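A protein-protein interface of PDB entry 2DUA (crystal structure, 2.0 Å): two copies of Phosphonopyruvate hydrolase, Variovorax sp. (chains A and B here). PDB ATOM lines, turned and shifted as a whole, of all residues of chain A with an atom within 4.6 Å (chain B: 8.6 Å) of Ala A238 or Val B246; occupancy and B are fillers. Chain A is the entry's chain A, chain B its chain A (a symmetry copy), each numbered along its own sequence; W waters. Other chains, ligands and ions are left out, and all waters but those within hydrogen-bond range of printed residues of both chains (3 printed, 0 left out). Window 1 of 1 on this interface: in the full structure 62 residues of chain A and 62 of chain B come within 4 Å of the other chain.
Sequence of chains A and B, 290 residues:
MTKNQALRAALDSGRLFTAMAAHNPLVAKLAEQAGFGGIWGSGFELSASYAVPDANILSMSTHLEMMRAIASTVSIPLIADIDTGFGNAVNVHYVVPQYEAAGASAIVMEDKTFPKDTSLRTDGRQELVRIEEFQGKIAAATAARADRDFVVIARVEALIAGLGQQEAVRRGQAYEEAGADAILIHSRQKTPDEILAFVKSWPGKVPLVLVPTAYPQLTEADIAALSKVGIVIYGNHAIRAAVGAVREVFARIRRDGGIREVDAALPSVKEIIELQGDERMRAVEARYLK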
ATOM      1  N   ALA A  21     -35.118  12.241  10.607  1.00  0.00           N
ATOM      2  CA  ALA A  21     -35.107  11.105  11.510  1.00  0.00           C
ATOM      3  C   ALA A  21     -34.559  11.490  12.898  1.00  0.00           C
ATOM      4  O   ALA A  21     -33.653  12.308  12.999  1.00  0.00           O
ATOM      5  CB  ALA A  21     -34.230   9.967  10.914  1.00  0.00           C
ATOM      6  N   HIS A  23     -33.669   9.499  16.838  1.00  0.00           N
ATOM      7  CA  HIS A  23     -33.757   8.279  17.653  1.00  0.00           C
ATOM      8  C   HIS A  23     -33.935   8.613  19.160  1.00  0.00           C
ATOM      9  O   HIS A  23     -34.115   7.718  20.010  1.00  0.00           O
ATOM     10  CB  HIS A  23     -32.556   7.360  17.390  1.00  0.00           C
ATOM     11  CG  HIS A  23     -31.249   8.077  17.420  1.00  0.00           C
ATOM     12  ND1 HIS A  23     -30.752   8.748  16.325  1.00  0.00           N
ATOM     13  CD2 HIS A  23     -30.320   8.200  18.394  1.00  0.00           C
ATOM     14  CE1 HIS A  23     -29.567   9.247  16.618  1.00  0.00           C
ATOM     15  NE2 HIS A  23     -29.280   8.926  17.867  1.00  0.00           N
ATOM     16  N   VAL A  27     -31.892  14.565  19.793  1.00  0.00           N
ATOM     17  CA  VAL A  27     -31.703  14.650  18.368  1.00  0.00           C
ATOM     18  C   VAL A  27     -32.923  15.357  17.742  1.00  0.00           C
ATOM     19  O   VAL A  27     -32.803  16.173  16.800  1.00  0.00           O
ATOM     20  CB  VAL A  27     -31.591  13.216  17.741  1.00  0.00           C
ATOM     21  CG1 VAL A  27     -31.734  13.313  16.199  1.00  0.00           C
ATOM     22  CG2 VAL A  27     -30.220  12.576  18.150  1.00  0.00           C
ATOM     23  N   LEU A  30     -32.543  19.030  18.245  1.00  0.00           N
ATOM     24  CA  LEU A  30     -31.527  19.569  17.320  1.00  0.00           C
ATOM     25  C   LEU A  30     -32.126  19.705  15.883  1.00  0.00           C
ATOM     26  O   LEU A  30     -31.767  20.626  15.159  1.00  0.00           O
ATOM     27  CB  LEU A  30     -30.310  18.642  17.300  1.00  0.00           C
ATOM     28  CG  LEU A  30     -29.560  18.640  18.659  1.00  0.00           C
ATOM     29  CD1 LEU A  30     -28.483  17.543  18.644  1.00  0.00           C
ATOM     30  CD2 LEU A  30     -28.948  20.041  18.932  1.00  0.00           C
ATOM     31  N   GLU A  45     -34.099   3.891  12.876  1.00  0.00           N
ATOM     32  CA  GLU A  45     -33.157   4.538  13.789  1.00  0.00           C
ATOM     33  C   GLU A  45     -33.325   4.075  15.237  1.00  0.00           C
ATOM     34  O   GLU A  45     -32.331   3.946  15.971  1.00  0.00           O
ATOM     35  CB  GLU A  45     -33.280   6.062  13.749  1.00  0.00           C
ATOM     36  CG  GLU A  45     -32.696   6.696  12.448  1.00  0.00           C
ATOM     37  CD  GLU A  45     -31.964   8.018  12.761  1.00  0.00           C
ATOM     38  OE1 GLU A  45     -32.118   8.501  13.891  1.00  0.00           O
ATOM     39  OE2 GLU A  45     -31.236   8.576  11.910  1.00  0.00           O
ATOM     40  N   ASN A 236     -32.317   8.190   7.893  1.00  0.00           N
ATOM     41  CA  ASN A 236     -31.424   7.595   8.888  1.00  0.00           C
ATOM     42  C   ASN A 236     -30.141   8.370   9.085  1.00  0.00           C
ATOM     43  O   ASN A 236     -29.153   7.816   9.521  1.00  0.00           O
ATOM     44  CB  ASN A 236     -31.058   6.212   8.400  1.00  0.00           C
ATOM     45  CG  ASN A 236     -30.514   6.237   6.989  1.00  0.00           C
ATOM     46  OD1 ASN A 236     -30.628   5.254   6.273  1.00  0.00           O
ATOM     47  ND2 ASN A 236     -29.943   7.360   6.565  1.00  0.00           N
ATOM     48  N   HIS A 237     -30.143   9.642   8.716  1.00  0.00           N
ATOM     49  CA  HIS A 237     -28.922  10.416   8.813  1.00  0.00           C
ATOM     50  C   HIS A 237     -28.495  10.781  10.220  1.00  0.00           C
ATOM     51  O   HIS A 237     -27.305  11.040  10.446  1.00  0.00           O
ATOM     52  CB  HIS A 237     -29.062  11.662   7.944  1.00  0.00           C
ATOM     53  CG  HIS A 237     -29.435  11.332   6.527  1.00  0.00           C
ATOM     54  ND1 HIS A 237     -30.739  11.113   6.134  1.00  0.00           N
ATOM     55  CD2 HIS A 237     -28.656  10.979   5.468  1.00  0.00           C
ATOM     56  CE1 HIS A 237     -30.743  10.620   4.901  1.00  0.00           C
ATOM     57  NE2 HIS A 237     -29.489  10.533   4.474  1.00  0.00           N
ATOM     58  N   ALA A 238     -29.433  10.790  11.173  1.00  0.00           N
ATOM     59  CA  ALA A 238     -29.061  11.190  12.538  1.00  0.00           C
ATOM     60  C   ALA A 238     -28.268  10.070  13.184  1.00  0.00           C
ATOM     61  O   ALA A 238     -27.226  10.319  13.817  1.00  0.00           O
ATOM     62  CB  ALA A 238     -30.313  11.490  13.386  1.00  0.00           C
ATOM     63  N   ILE A 239     -28.752   8.838  13.028  1.00  0.00           N
ATOM     64  CA  ILE A 239     -28.039   7.739  13.645  1.00  0.00           C
ATOM     65  C   ILE A 239     -26.684   7.580  12.935  1.00  0.00           C
ATOM     66  O   ILE A 239     -25.704   7.245  13.562  1.00  0.00           O
ATOM     67  CB  ILE A 239     -28.900   6.370  13.631  1.00  0.00           C
ATOM     68  CG1 ILE A 239     -28.336   5.365  14.638  1.00  0.00           C
ATOM     69  CG2 ILE A 239     -28.908   5.768  12.275  1.00  0.00           C
ATOM     70  CD1 ILE A 239     -28.576   5.773  16.070  1.00  0.00           C
ATOM     71  N   ARG A 240     -26.628   7.846  11.627  1.00  0.00           N
ATOM     72  CA  ARG A 240     -25.350   7.675  10.923  1.00  0.00           C
ATOM     73  C   ARG A 240     -24.337   8.739  11.373  1.00  0.00           C
ATOM     74  O   ARG A 240     -23.174   8.412  11.631  1.00  0.00           O
ATOM     75  CB  ARG A 240     -25.564   7.702   9.404  1.00  0.00           C
ATOM     76  CG  ARG A 240     -26.209   6.371   8.902  1.00  0.00           C
ATOM     77  CD  ARG A 240     -26.891   6.609   7.513  1.00  0.00           C
ATOM     78  NE  ARG A 240     -25.890   6.819   6.445  1.00  0.00           N
ATOM     79  CZ  ARG A 240     -26.206   7.331   5.252  1.00  0.00           C
ATOM     80  NH1 ARG A 240     -27.474   7.677   4.993  1.00  0.00           N
ATOM     81  NH2 ARG A 240     -25.274   7.484   4.331  1.00  0.00           N
ATOM     82  N   ALA A 241     -24.793   9.979  11.495  1.00  0.00           N
ATOM     83  CA  ALA A 241     -23.921  11.056  11.927  1.00  0.00           C
ATOM     84  C   ALA A 241     -23.397  10.740  13.356  1.00  0.00           C
ATOM     85  O   ALA A 241     -22.192  10.877  13.639  1.00  0.00           O
ATOM     86  CB  ALA A 241     -24.706  12.429  11.910  1.00  0.00           C
ATOM     87  N   ALA A 242     -24.296  10.296  14.238  1.00  0.00           N
ATOM     88  CA  ALA A 242     -23.917  10.005  15.620  1.00  0.00           C
ATOM     89  C   ALA A 242     -22.917   8.865  15.668  1.00  0.00           C
ATOM     90  O   ALA A 242     -21.893   8.962  16.376  1.00  0.00           O
ATOM     91  CB  ALA A 242     -25.160   9.653  16.486  1.00  0.00           C
ATOM     92  N   HIS B  23     -25.292   6.360  26.253  1.00  0.00           N
ATOM     93  CA  HIS B  23     -26.700   6.712  26.480  1.00  0.00           C
ATOM     94  C   HIS B  23     -27.658   5.720  25.764  1.00  0.00           C
ATOM     95  O   HIS B  23     -28.896   5.792  25.901  1.00  0.00           O
ATOM     96  CB  HIS B  23     -26.966   8.173  26.092  1.00  0.00           C
ATOM     97  CG  HIS B  23     -26.405   8.540  24.760  1.00  0.00           C
ATOM     98  ND1 HIS B  23     -25.092   8.918  24.595  1.00  0.00           N
ATOM     99  CD2 HIS B  23     -26.981   8.622  23.540  1.00  0.00           C
ATOM    100  CE1 HIS B  23     -24.881   9.228  23.330  1.00  0.00           C
ATOM    101  NE2 HIS B  23     -26.013   9.060  22.669  1.00  0.00           N
ATOM    102  N   LEU B  26     -26.199   1.053  21.340  1.00  0.00           N
ATOM    103  CA  LEU B  26     -25.327   1.179  20.165  1.00  0.00           C
ATOM    104  C   LEU B  26     -24.023   1.878  20.562  1.00  0.00           C
ATOM    105  O   LEU B  26     -22.942   1.448  20.209  1.00  0.00           O
ATOM    106  CB  LEU B  26     -26.022   1.982  19.043  1.00  0.00           C
ATOM    107  CG  LEU B  26     -25.190   2.265  17.766  1.00  0.00           C
ATOM    108  CD1 LEU B  26     -24.803   1.000  17.124  1.00  0.00           C
ATOM    109  CD2 LEU B  26     -26.028   3.098  16.788  1.00  0.00           C
ATOM    110  N   ALA B 238     -19.721  10.755  25.088  1.00  0.00           N
ATOM    111  CA  ALA B 238     -20.474  10.134  23.988  1.00  0.00           C
ATOM    112  C   ALA B 238     -21.604  11.060  23.577  1.00  0.00           C
ATOM    113  O   ALA B 238     -21.827  11.285  22.374  1.00  0.00           O
ATOM    114  CB  ALA B 238     -21.055   8.772  24.417  1.00  0.00           C
ATOM    115  N   ILE B 239     -22.316  11.597  24.566  1.00  0.00           N
ATOM    116  CA  ILE B 239     -23.418  12.471  24.220  1.00  0.00           C
ATOM    117  C   ILE B 239     -22.843  13.749  23.587  1.00  0.00           C
ATOM    118  O   ILE B 239     -23.440  14.307  22.692  1.00  0.00           O
ATOM    119  CB  ILE B 239     -24.364  12.792  25.492  1.00  0.00           C
ATOM    120  CG1 ILE B 239     -25.719  13.339  25.036  1.00  0.00           C
ATOM    121  CG2 ILE B 239     -23.711  13.768  26.399  1.00  0.00           C
ATOM    122  CD1 ILE B 239     -26.577  12.293  24.369  1.00  0.00           C
ATOM    123  N   ARG B 240     -21.668  14.197  24.037  1.00  0.00           N
ATOM    124  CA  ARG B 240     -21.113  15.431  23.464  1.00  0.00           C
ATOM    125  C   ARG B 240     -20.681  15.204  22.007  1.00  0.00           C
ATOM    126  O   ARG B 240     -20.972  16.037  21.142  1.00  0.00           O
ATOM    127  CB  ARG B 240     -19.955  15.951  24.326  1.00  0.00           C
ATOM    128  CG  ARG B 240     -20.482  16.602  25.643  1.00  0.00           C
ATOM    129  CD  ARG B 240     -19.335  16.634  26.708  1.00  0.00           C
ATOM    130  NE  ARG B 240     -18.287  17.613  26.349  1.00  0.00           N
ATOM    131  CZ  ARG B 240     -17.079  17.617  26.922  1.00  0.00           C
ATOM    132  NH1 ARG B 240     -16.785  16.706  27.859  1.00  0.00           N
ATOM    133  NH2 ARG B 240     -16.186  18.524  26.571  1.00  0.00           N
ATOM    134  N   ALA B 241     -20.029  14.078  21.749  1.00  0.00           N
ATOM    135  CA  ALA B 241     -19.588  13.762  20.402  1.00  0.00           C
ATOM    136  C   ALA B 241     -20.831  13.662  19.474  1.00  0.00           C
ATOM    137  O   ALA B 241     -20.842  14.218  18.359  1.00  0.00           O
ATOM    138  CB  ALA B 241     -18.778  12.404  20.402  1.00  0.00           C
ATOM    139  N   ALA B 242     -21.876  12.978  19.946  1.00  0.00           N
ATOM    140  CA  ALA B 242     -23.081  12.790  19.139  1.00  0.00           C
ATOM    141  C   ALA B 242     -23.746  14.125  18.858  1.00  0.00           C
ATOM    142  O   ALA B 242     -24.124  14.402  17.700  1.00  0.00           O
ATOM    143  CB  ALA B 242     -24.089  11.837  19.841  1.00  0.00           C
ATOM    144  N   VAL B 243     -23.882  14.962  19.890  1.00  0.00           N
ATOM    145  CA  VAL B 243     -24.518  16.267  19.671  1.00  0.00           C
ATOM    146  C   VAL B 243     -23.742  17.106  18.621  1.00  0.00           C
ATOM    147  O   VAL B 243     -24.335  17.732  17.721  1.00  0.00           O
ATOM    148  CB  VAL B 243     -24.676  17.098  21.024  1.00  0.00           C
ATOM    149  CG1 VAL B 243     -24.883  18.538  20.724  1.00  0.00           C
ATOM    150  CG2 VAL B 243     -25.879  16.585  21.897  1.00  0.00           C
ATOM    151  N   GLY B 244     -22.425  17.123  18.734  1.00  0.00           N
ATOM    152  CA  GLY B 244     -21.631  17.903  17.795  1.00  0.00           C
ATOM    153  C   GLY B 244     -21.806  17.472  16.346  1.00  0.00           C
ATOM    154  O   GLY B 244     -22.023  18.328  15.456  1.00  0.00           O
ATOM    155  N   ALA B 245     -21.772  16.171  16.095  1.00  0.00           N
ATOM    156  CA  ALA B 245     -21.902  15.708  14.701  1.00  0.00           C
ATOM    157  C   ALA B 245     -23.299  15.822  14.163  1.00  0.00           C
ATOM    158  O   ALA B 245     -23.494  16.087  12.985  1.00  0.00           O
ATOM    159  CB  ALA B 245     -21.461  14.283  14.565  1.00  0.00           C
ATOM    160  N   VAL B 246     -24.286  15.571  15.019  1.00  0.00           N
ATOM    161  CA  VAL B 246     -25.675  15.647  14.555  1.00  0.00           C
ATOM    162  C   VAL B 246     -26.032  17.067  14.225  1.00  0.00           C
ATOM    163  O   VAL B 246     -26.638  17.364  13.161  1.00  0.00           O
ATOM    164  CB  VAL B 246     -26.657  15.123  15.639  1.00  0.00           C
ATOM    165  CG1 VAL B 246     -28.092  15.554  15.291  1.00  0.00           C
ATOM    166  CG2 VAL B 246     -26.504  13.592  15.746  1.00  0.00           C
ATOM    167  N   ARG B 247     -25.668  17.967  15.130  1.00  0.00           N
ATOM    168  CA  ARG B 247     -25.951  19.385  14.917  1.00  0.00           C
ATOM    169  C   ARG B 247     -25.249  19.879  13.631  1.00  0.00           C
ATOM    170  O   ARG B 247     -25.782  20.690  12.870  1.00  0.00           O
ATOM    171  CB  ARG B 247     -25.429  20.150  16.126  1.00  0.00           C
ATOM    172  CG  ARG B 247     -25.655  21.591  16.152  1.00  0.00           C
ATOM    173  CD  ARG B 247     -25.247  22.091  17.577  1.00  0.00           C
ATOM    174  NE  ARG B 247     -23.809  21.918  17.818  1.00  0.00           N
ATOM    175  CZ  ARG B 247     -23.198  22.334  18.928  1.00  0.00           C
ATOM    176  NH1 ARG B 247     -23.920  22.922  19.894  1.00  0.00           N
ATOM    177  NH2 ARG B 247     -21.873  22.242  19.034  1.00  0.00           N
ATOM    178  N   GLU B 248     -24.027  19.406  13.405  1.00  0.00           N
ATOM    179  CA  GLU B 248     -23.323  19.844  12.209  1.00  0.00           C
ATOM    180  C   GLU B 248     -23.908  19.277  10.912  1.00  0.00           C
ATOM    181  O   GLU B 248     -24.030  19.994   9.942  1.00  0.00           O
ATOM    182  CB  GLU B 248     -21.862  19.472  12.313  1.00  0.00           C
ATOM    183  CG  GLU B 248     -20.993  20.323  11.441  1.00  0.00           C
ATOM    184  CD  GLU B 248     -20.116  19.450  10.621  1.00  0.00           C
ATOM    185  OE1 GLU B 248     -20.648  18.885   9.619  1.00  0.00           O
ATOM    186  OE2 GLU B 248     -18.911  19.304  10.998  1.00  0.00           O
ATOM    187  N   VAL B 249     -24.273  17.999  10.904  1.00  0.00           N
ATOM    188  CA  VAL B 249     -24.855  17.390   9.718  1.00  0.00           C
ATOM    189  C   VAL B 249     -26.232  17.982   9.427  1.00  0.00           C
ATOM    190  O   VAL B 249     -26.578  18.197   8.254  1.00  0.00           O
ATOM    191  CB  VAL B 249     -24.978  15.864   9.884  1.00  0.00           C
ATOM    192  CG1 VAL B 249     -25.743  15.262   8.734  1.00  0.00           C
ATOM    193  CG2 VAL B 249     -23.577  15.246   9.905  1.00  0.00           C
ATOM    194  N   PHE B 250     -27.006  18.282  10.469  1.00  0.00           N
ATOM    195  CA  PHE B 250     -28.333  18.886  10.259  1.00  0.00           C
ATOM    196  C   PHE B 250     -28.188  20.298   9.641  1.00  0.00           C
ATOM    197  O   PHE B 250     -28.962  20.705   8.733  1.00  0.00           O
ATOM    198  CB  PHE B 250     -29.136  18.996  11.570  1.00  0.00           C
ATOM    199  CG  PHE B 250     -29.664  17.666  12.117  1.00  0.00           C
ATOM    200  CD1 PHE B 250     -29.534  16.487  11.395  1.00  0.00           C
ATOM    201  CD2 PHE B 250     -30.346  17.618  13.348  1.00  0.00           C
ATOM    202  CE1 PHE B 250     -30.087  15.255  11.879  1.00  0.00           C
ATOM    203  CE2 PHE B 250     -30.918  16.371  13.853  1.00  0.00           C
ATOM    204  CZ  PHE B 250     -30.778  15.199  13.092  1.00  0.00           C
ATOM    205  N   ALA B 251     -27.205  21.047  10.118  1.00  0.00           N
ATOM    206  CA  ALA B 251     -27.002  22.404   9.590  1.00  0.00           C
ATOM    207  C   ALA B 251     -26.532  22.363   8.119  1.00  0.00           C
ATOM    208  O   ALA B 251     -26.952  23.199   7.315  1.00  0.00           O
ATOM    209  CB  ALA B 251     -26.013  23.173  10.476  1.00  0.00           C
ATOM    210  N   ARG B 252     -25.683  21.391   7.781  1.00  0.00           N
ATOM    211  CA  ARG B 252     -25.193  21.232   6.438  1.00  0.00           C
ATOM    212  C   ARG B 252     -26.353  20.837   5.525  1.00  0.00           C
ATOM    213  O   ARG B 252     -26.481  21.371   4.434  1.00  0.00           O
ATOM    214  CB  ARG B 252     -24.090  20.189   6.380  1.00  0.00           C
ATOM    215  CG  ARG B 252     -22.748  20.702   6.934  1.00  0.00           C
ATOM    216  CD  ARG B 252     -21.577  19.675   6.818  1.00  0.00           C
ATOM    217  NE  ARG B 252     -21.274  19.288   5.429  1.00  0.00           N
ATOM    218  CZ  ARG B 252     -20.585  18.186   5.082  1.00  0.00           C
ATOM    219  NH1 ARG B 252     -20.126  17.357   6.008  1.00  0.00           N
ATOM    220  NH2 ARG B 252     -20.365  17.896   3.798  1.00  0.00           N
ATOM    221  N   ILE B 253     -27.192  19.903   5.930  1.00  0.00           N
ATOM    222  CA  ILE B 253     -28.328  19.522   5.078  1.00  0.00           C
ATOM    223  C   ILE B 253     -29.262  20.728   4.810  1.00  0.00           C
ATOM    224  O   ILE B 253     -29.705  20.957   3.683  1.00  0.00           O
ATOM    225  CB  ILE B 253     -29.122  18.356   5.732  1.00  0.00           C
ATOM    226  CG1 ILE B 253     -28.242  17.102   5.753  1.00  0.00           C
ATOM    227  CG2 ILE B 253     -30.458  18.110   4.992  1.00  0.00           C
ATOM    228  CD1 ILE B 253     -28.879  15.853   6.461  1.00  0.00           C
ATOM    229  N   VAL B 262     -23.188  15.844   2.001  1.00  0.00           N
ATOM    230  CA  VAL B 262     -22.931  15.157   3.260  1.00  0.00           C
ATOM    231  C   VAL B 262     -22.923  13.629   3.284  1.00  0.00           C
ATOM    232  O   VAL B 262     -22.242  13.022   4.138  1.00  0.00           O
ATOM    233  CB  VAL B 262     -23.911  15.661   4.313  1.00  0.00           C
ATOM    234  CG1 VAL B 262     -25.150  14.822   4.268  1.00  0.00           C
ATOM    235  CG2 VAL B 262     -23.243  15.660   5.681  1.00  0.00           C
ATOM    236  N   LEU B 266     -20.630  10.353   5.776  1.00  0.00           N
ATOM    237  CA  LEU B 266     -21.288   9.497   6.785  1.00  0.00           C
ATOM    238  C   LEU B 266     -21.015   7.986   6.713  1.00  0.00           C
ATOM    239  O   LEU B 266     -20.722   7.446   5.640  1.00  0.00           O
ATOM    240  CB  LEU B 266     -22.821   9.640   6.633  1.00  0.00           C
ATOM    241  CG  LEU B 266     -23.441  11.026   6.760  1.00  0.00           C
ATOM    242  CD1 LEU B 266     -24.972  11.040   6.397  1.00  0.00           C
ATOM    243  CD2 LEU B 266     -23.200  11.434   8.221  1.00  0.00           C
ATOM    244  N   PRO B 267     -21.153   7.267   7.861  1.00  0.00           N
ATOM    245  CA  PRO B 267     -20.966   5.813   7.826  1.00  0.00           C
ATOM    246  C   PRO B 267     -22.111   5.361   6.908  1.00  0.00           C
ATOM    247  O   PRO B 267     -23.155   6.045   6.831  1.00  0.00           O
ATOM    248  CB  PRO B 267     -21.298   5.434   9.336  1.00  0.00           C
ATOM    249  CG  PRO B 267     -20.761   6.600  10.092  1.00  0.00           C
ATOM    250  CD  PRO B 267     -21.194   7.820   9.240  1.00  0.00           C
ATOM    251  N   ILE B 272     -24.439   0.482   9.652  1.00  0.00           N
ATOM    252  CA  ILE B 272     -25.395   0.502  10.782  1.00  0.00           C
ATOM    253  C   ILE B 272     -26.049  -0.872  10.862  1.00  0.00           C
ATOM    254  O   ILE B 272     -26.172  -1.429  11.952  1.00  0.00           O
ATOM    255  CB  ILE B 272     -26.518   1.571  10.568  1.00  0.00           C
ATOM    256  CG1 ILE B 272     -25.878   2.942  10.288  1.00  0.00           C
ATOM    257  CG2 ILE B 272     -27.459   1.574  11.761  1.00  0.00           C
ATOM    258  CD1 ILE B 272     -24.855   3.379  11.361  1.00  0.00           C
HETATM  259  O   HOH W   1     -22.497   7.171   3.451  1.00  0.00           O
HETATM  260  O   HOH W   2     -26.623   7.701  19.692  1.00  0.00           O
HETATM  261  O   HOH W   3     -27.929  10.715  20.327  1.00  0.00           O
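The guanidinium group (NE) of Arg A240 sits at hydrogen-bond distance from the backbone carbonyl oxygen (O) of Pro B267 (2.9 Å).
The side-chain carboxylate (OE2) of Glu A45 is in hydrogen-bond range of the backbone NH (N) of Ala A238 (2.9 Å).
OE2 of Glu A45 lies within hydrogen-bond range of N of Ile A239 (2.7 Å).
NH1 of Arg A240 lies close to ND2 of Asn A236 (2.9 Å).
Among the printed residues, pairs that only touch across the chains: Val A27 with Phe B250 (3.5 Å), Leu A30 with Val B246 (3.9 Å), Leu A30 with Phe B250 (3.7 Å), His A237 with Leu B266 (3.8 Å), Ala A238 with Val B246 (3.9 Å), Ala A238 with Phe B250 (3.7 Å), Ile A239 with Leu B26 (3.8 Å), Arg A240 with Leu B266 (3.996 Å), Arg A240 with Ile B272 (3.7 Å), Ala A241 with Ala B245 (3.6 Å), Ala A241 with Val B249 (3.6 Å) and Ala A241 with Leu B266 (3.8 Å).
Of the printed residues of chain B, Val A27 touches Phe B250 (3.5 Å).
Of the printed residues of chain B, Arg A240 touches Leu B266 (3.996 Å), Pro B267 (2.9 Å) and Ile B272 (3.7 Å).
Of chain A, only Leu A30 and Ala A238 come within 4 Å of Val B246.
Printed residues of chain A within 4 Å of Val B249: Ala A241 (3.6 Å).
Printed residues of chain A within 4 Å of Pro B267: Arg A240.
The nearest residue of chain A that does not touch Val B246 is Ala A242 (4.2 Å).
The nearest printed residue of chain B that does not touch His A237 is Ile B253 (4.4 Å).
Along chain B the printed residues that touch a printed residue of chain A span positions 26 to 272.
Among the printed residues, no Asp or Glu carboxylate lies within 4 Å of a Lys or Arg side-chain nitrogen of the other chain.
Positions printed for both chains: 23, 238, 239, 240, 241 and 242.
Of the 13 pairs that touch across the chains among the printed residues, none has its exchanged pair printed and touching as well.
Water W1 bridges the backbone carbonyl oxygen of Leu B266 (2.8 Å) and the guanidinium group of Arg A240 (2.9 Å).
Water W3 bridges NE2 of His A23 (3.3 Å) and NE2 of His B23 (3.4 Å).
Water W2 bridges NE2 of His B23 and NE2 of His A23.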
